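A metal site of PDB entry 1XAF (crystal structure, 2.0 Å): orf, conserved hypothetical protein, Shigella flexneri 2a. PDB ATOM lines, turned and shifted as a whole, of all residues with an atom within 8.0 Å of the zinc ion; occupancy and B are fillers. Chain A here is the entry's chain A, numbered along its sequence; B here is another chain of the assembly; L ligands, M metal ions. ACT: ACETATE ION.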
ATOM      1  N   GLN A  72       1.046  31.051 -11.011  1.00  0.00           N
ATOM      2  CA  GLN A  72       1.476  31.539 -12.333  1.00  0.00           C
ATOM      3  C   GLN A  72       0.517  32.583 -12.867  1.00  0.00           C
ATOM      4  O   GLN A  72      -0.686  32.334 -12.939  1.00  0.00           O
ATOM      5  CB  GLN A  72       1.569  30.382 -13.345  1.00  0.00           C
ATOM      6  CG  GLN A  72       2.598  29.321 -12.939  1.00  0.00           C
ATOM      7  CD  GLN A  72       2.499  28.028 -13.750  1.00  0.00           C
ATOM      8  OE1 GLN A  72       1.741  27.921 -14.732  1.00  0.00           O
ATOM      9  NE2 GLN A  72       3.251  27.055 -13.338  1.00  0.00           N
ATOM     10  N   VAL A  73       1.058  33.714 -13.291  1.00  0.00           N
ATOM     11  CA  VAL A  73       0.212  34.862 -13.702  1.00  0.00           C
ATOM     12  C   VAL A  73       0.501  35.280 -15.175  1.00  0.00           C
ATOM     13  O   VAL A  73       0.057  36.345 -15.630  1.00  0.00           O
ATOM     14  CB  VAL A  73       0.368  36.045 -12.693  1.00  0.00           C
ATOM     15  CG1 VAL A  73      -0.248  35.719 -11.350  1.00  0.00           C
ATOM     16  CG2 VAL A  73       1.808  36.419 -12.494  1.00  0.00           C
ATOM     17  N   HIS A  74       1.243  34.439 -15.898  1.00  0.00           N
ATOM     18  CA  HIS A  74       1.627  34.732 -17.289  1.00  0.00           C
ATOM     19  C   HIS A  74       2.515  35.955 -17.427  1.00  0.00           C
ATOM     20  O   HIS A  74       2.515  36.604 -18.474  1.00  0.00           O
ATOM     21  CB  HIS A  74       0.401  34.809 -18.215  1.00  0.00           C
ATOM     22  CG  HIS A  74      -0.186  33.470 -18.514  1.00  0.00           C
ATOM     23  ND1 HIS A  74      -1.008  32.809 -17.636  1.00  0.00           N
ATOM     24  CD2 HIS A  74      -0.021  32.628 -19.565  1.00  0.00           C
ATOM     25  CE1 HIS A  74      -1.363  31.641 -18.142  1.00  0.00           C
ATOM     26  NE2 HIS A  74      -0.791  31.510 -19.321  1.00  0.00           N
ATOM     27  N   ASP A  92       6.356  33.122 -12.794  1.00  0.00           N
ATOM     28  CA  ASP A  92       6.145  32.177 -13.889  1.00  0.00           C
ATOM     29  C   ASP A  92       7.378  31.328 -14.162  1.00  0.00           C
ATOM     30  O   ASP A  92       7.384  30.561 -15.117  1.00  0.00           O
ATOM     31  CB  ASP A  92       5.617  32.882 -15.124  1.00  0.00           C
ATOM     32  CG  ASP A  92       4.129  33.283 -14.988  1.00  0.00           C
ATOM     33  OD1 ASP A  92       3.245  32.498 -15.445  1.00  0.00           O
ATOM     34  OD2 ASP A  92       3.846  34.374 -14.415  1.00  0.00           O
ATOM     35  N   MET A 106       3.280  24.403 -14.577  1.00  0.00           N
ATOM     36  CA  MET A 106       2.019  23.806 -14.958  1.00  0.00           C
ATOM     37  C   MET A 106       1.552  24.437 -16.269  1.00  0.00           C
ATOM     38  O   MET A 106       1.504  25.651 -16.375  1.00  0.00           O
ATOM     39  CB  MET A 106       1.015  24.097 -13.830  1.00  0.00           C
ATOM     40  CG  MET A 106      -0.429  24.056 -14.220  1.00  0.00           C
ATOM     41  SD  MET A 106      -1.348  23.224 -12.780  1.00  0.00           S
ATOM     42  CE  MET A 106      -0.316  21.503 -13.036  1.00  0.00           C
ATOM     43  N   THR A 107       1.216  23.622 -17.267  1.00  0.00           N
ATOM     44  CA  THR A 107       0.965  24.128 -18.625  1.00  0.00           C
ATOM     45  C   THR A 107      -0.111  23.270 -19.297  1.00  0.00           C
ATOM     46  O   THR A 107      -0.369  22.149 -18.870  1.00  0.00           O
ATOM     47  CB  THR A 107       2.250  24.077 -19.540  1.00  0.00           C
ATOM     48  OG1 THR A 107       2.591  22.714 -19.815  1.00  0.00           O
ATOM     49  CG2 THR A 107       3.457  24.817 -18.915  1.00  0.00           C
ATOM     50  N   ALA A 108      -0.729  23.817 -20.339  1.00  0.00           N
ATOM     51  CA  ALA A 108      -1.565  23.038 -21.296  1.00  0.00           C
ATOM     52  C   ALA A 108      -1.683  23.845 -22.574  1.00  0.00           C
ATOM     53  O   ALA A 108      -2.783  24.227 -22.978  1.00  0.00           O
ATOM     54  CB  ALA A 108      -2.942  22.724 -20.705  1.00  0.00           C
ATOM     55  N   ASP A 109      -0.514  24.136 -23.147  1.00  0.00           N
ATOM     56  CA  ASP A 109      -0.287  24.898 -24.395  1.00  0.00           C
ATOM     57  C   ASP A 109       0.918  25.855 -24.291  1.00  0.00           C
ATOM     58  O   ASP A 109       1.683  25.970 -25.259  1.00  0.00           O
ATOM     59  CB  ASP A 109      -1.472  25.765 -24.822  1.00  0.00           C
ATOM     60  CG  ASP A 109      -2.503  25.027 -25.664  1.00  0.00           C
ATOM     61  OD1 ASP A 109      -2.328  23.864 -26.101  1.00  0.00           O
ATOM     62  OD2 ASP A 109      -3.519  25.680 -25.912  1.00  0.00           O
ATOM     63  N   CYS A 110       1.062  26.564 -23.142  1.00  0.00           N
ATOM     64  CA  CYS A 110       2.248  27.404 -22.964  1.00  0.00           C
ATOM     65  C   CYS A 110       3.528  26.591 -22.962  1.00  0.00           C
ATOM     66  O   CYS A 110       3.535  25.408 -22.648  1.00  0.00           O
ATOM     67  CB  CYS A 110       2.168  28.305 -21.740  1.00  0.00           C
ATOM     68  SG  CYS A 110       0.736  29.453 -21.782  1.00  0.00           S
ATOM     69  N   LEU A 111       4.601  27.225 -23.360  1.00  0.00           N
ATOM     70  CA  LEU A 111       5.876  26.572 -23.441  1.00  0.00           C
ATOM     71  C   LEU A 111       6.472  26.334 -22.067  1.00  0.00           C
ATOM     72  O   LEU A 111       6.702  27.305 -21.327  1.00  0.00           O
ATOM     73  CB  LEU A 111       6.819  27.474 -24.247  1.00  0.00           C
ATOM     74  CG  LEU A 111       8.260  26.994 -24.359  1.00  0.00           C
ATOM     75  CD1 LEU A 111       8.238  25.715 -25.116  1.00  0.00           C
ATOM     76  CD2 LEU A 111       9.086  28.075 -25.158  1.00  0.00           C
ATOM     77  N   HIS A 127       7.389  28.676 -17.095  1.00  0.00           N
ATOM     78  CA  HIS A 127       6.123  28.667 -17.800  1.00  0.00           C
ATOM     79  C   HIS A 127       6.109  29.891 -18.753  1.00  0.00           C
ATOM     80  O   HIS A 127       5.918  31.023 -18.358  1.00  0.00           O
ATOM     81  CB  HIS A 127       4.927  28.644 -16.818  1.00  0.00           C
ATOM     82  CG  HIS A 127       3.624  29.154 -17.380  1.00  0.00           C
ATOM     83  ND1 HIS A 127       3.060  30.350 -16.978  1.00  0.00           N
ATOM     84  CD2 HIS A 127       2.775  28.635 -18.305  1.00  0.00           C
ATOM     85  CE1 HIS A 127       1.929  30.548 -17.617  1.00  0.00           C
ATOM     86  NE2 HIS A 127       1.733  29.521 -18.443  1.00  0.00           N
ATOM     87  N   ALA A 128       6.383  29.623 -20.021  1.00  0.00           N
ATOM     88  CA  ALA A 128       6.556  30.733 -20.942  1.00  0.00           C
ATOM     89  C   ALA A 128       5.349  30.882 -21.858  1.00  0.00           C
ATOM     90  O   ALA A 128       5.328  30.319 -22.949  1.00  0.00           O
ATOM     91  CB  ALA A 128       7.871  30.550 -21.744  1.00  0.00           C
ATOM     92  N   GLY A 129       4.321  31.590 -21.380  1.00  0.00           N
ATOM     93  CA  GLY A 129       3.264  32.094 -22.250  1.00  0.00           C
ATOM     94  C   GLY A 129       3.860  33.092 -23.225  1.00  0.00           C
ATOM     95  O   GLY A 129       4.977  33.570 -22.998  1.00  0.00           O
ATOM     96  N   TRP A 130       3.158  33.403 -24.306  1.00  0.00           N
ATOM     97  CA  TRP A 130       3.698  34.374 -25.272  1.00  0.00           C
ATOM     98  C   TRP A 130       4.032  35.746 -24.652  1.00  0.00           C
ATOM     99  O   TRP A 130       5.027  36.358 -25.034  1.00  0.00           O
ATOM    100  CB  TRP A 130       2.798  34.563 -26.496  1.00  0.00           C
ATOM    101  CG  TRP A 130       1.560  35.432 -26.294  1.00  0.00           C
ATOM    102  CD1 TRP A 130       0.296  35.003 -25.974  1.00  0.00           C
ATOM    103  CD2 TRP A 130       1.473  36.861 -26.474  1.00  0.00           C
ATOM    104  NE1 TRP A 130      -0.569  36.087 -25.908  1.00  0.00           N
ATOM    105  CE2 TRP A 130       0.128  37.233 -26.208  1.00  0.00           C
ATOM    106  CE3 TRP A 130       2.408  37.870 -26.786  1.00  0.00           C
ATOM    107  CZ2 TRP A 130      -0.314  38.580 -26.282  1.00  0.00           C
ATOM    108  CZ3 TRP A 130       1.968  39.203 -26.844  1.00  0.00           C
ATOM    109  CH2 TRP A 130       0.623  39.534 -26.593  1.00  0.00           C
ATOM    110  N   TYR A 230      -5.472  23.808 -23.774  1.00  0.00           N
ATOM    111  CA  TYR A 230      -6.468  24.834 -23.452  1.00  0.00           C
ATOM    112  C   TYR A 230      -7.156  25.454 -24.682  1.00  0.00           C
ATOM    113  O   TYR A 230      -8.366  25.712 -24.687  1.00  0.00           O
ATOM    114  CB  TYR A 230      -5.834  25.930 -22.613  1.00  0.00           C
ATOM    115  CG  TYR A 230      -6.762  27.045 -22.203  1.00  0.00           C
ATOM    116  CD1 TYR A 230      -7.607  26.926 -21.099  1.00  0.00           C
ATOM    117  CD2 TYR A 230      -6.747  28.264 -22.882  1.00  0.00           C
ATOM    118  CE1 TYR A 230      -8.440  27.952 -20.729  1.00  0.00           C
ATOM    119  CE2 TYR A 230      -7.582  29.313 -22.523  1.00  0.00           C
ATOM    120  CZ  TYR A 230      -8.427  29.146 -21.441  1.00  0.00           C
ATOM    121  OH  TYR A 230      -9.230  30.187 -21.070  1.00  0.00           O
ATOM    122  N   ARG A 238      -4.332  19.726 -16.846  1.00  0.00           N
ATOM    123  CA  ARG A 238      -3.035  20.394 -16.949  1.00  0.00           C
ATOM    124  C   ARG A 238      -1.961  19.359 -16.786  1.00  0.00           C
ATOM    125  O   ARG A 238      -2.131  18.445 -15.971  1.00  0.00           O
ATOM    126  CB  ARG A 238      -2.850  21.444 -15.826  1.00  0.00           C
ATOM    127  CG  ARG A 238      -3.835  22.594 -15.882  1.00  0.00           C
ATOM    128  CD  ARG A 238      -3.556  23.513 -17.141  1.00  0.00           C
ATOM    129  NE  ARG A 238      -4.490  24.649 -17.175  1.00  0.00           N
ATOM    130  CZ  ARG A 238      -5.753  24.639 -17.583  1.00  0.00           C
ATOM    131  NH1 ARG A 238      -6.338  23.526 -18.039  1.00  0.00           N
ATOM    132  NH2 ARG A 238      -6.453  25.770 -17.555  1.00  0.00           N
ATOM    133  N   ASN B 224      -7.050  35.484 -19.888  1.00  0.00           N
ATOM    134  CA  ASN B 224      -6.073  36.572 -19.918  1.00  0.00           C
ATOM    135  C   ASN B 224      -5.912  37.253 -21.264  1.00  0.00           C
ATOM    136  O   ASN B 224      -5.444  38.386 -21.342  1.00  0.00           O
ATOM    137  CB  ASN B 224      -4.742  36.148 -19.284  1.00  0.00           C
ATOM    138  CG  ASN B 224      -4.202  34.875 -19.846  1.00  0.00           C
ATOM    139  OD1 ASN B 224      -3.783  34.821 -20.992  1.00  0.00           O
ATOM    140  ND2 ASN B 224      -4.189  33.830 -19.026  1.00  0.00           N
HETATM  141  C   ACT L   1      -1.560  27.130 -19.847  1.00  0.00           C
HETATM  142  O   ACT L   1      -0.590  26.535 -20.386  1.00  0.00           O
HETATM  143  OXT ACT L   1      -1.357  28.265 -19.288  1.00  0.00           O
HETATM  144  CH3 ACT L   1      -2.935  26.517 -19.834  1.00  0.00           C
HETATM  145 ZN    ZN M   1       0.092  29.557 -19.755  1.00  0.00          ZN
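The nearest printed residue that does not touch the zinc ion is Gly 129 (4.8 Å).
A ring nitrogen (ND1) of His 127 is in hydrogen-bond range of the side-chain carboxylate (OD1) of Asp 92.
The backbone NH (N) of His 74 lies within hydrogen-bond range of the side-chain carboxylate (OD1) of Asp 92 (2.8 Å).
The zinc ion is bound by an oxygen (OXT) of the ligand (2.0 Å), a ring nitrogen (NE2) of His 127 (2.1 Å), the side-chain sulfur (SG) of Cys 110 (2.1 Å) and a ring nitrogen (NE2) of His 74 (2.2 Å).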
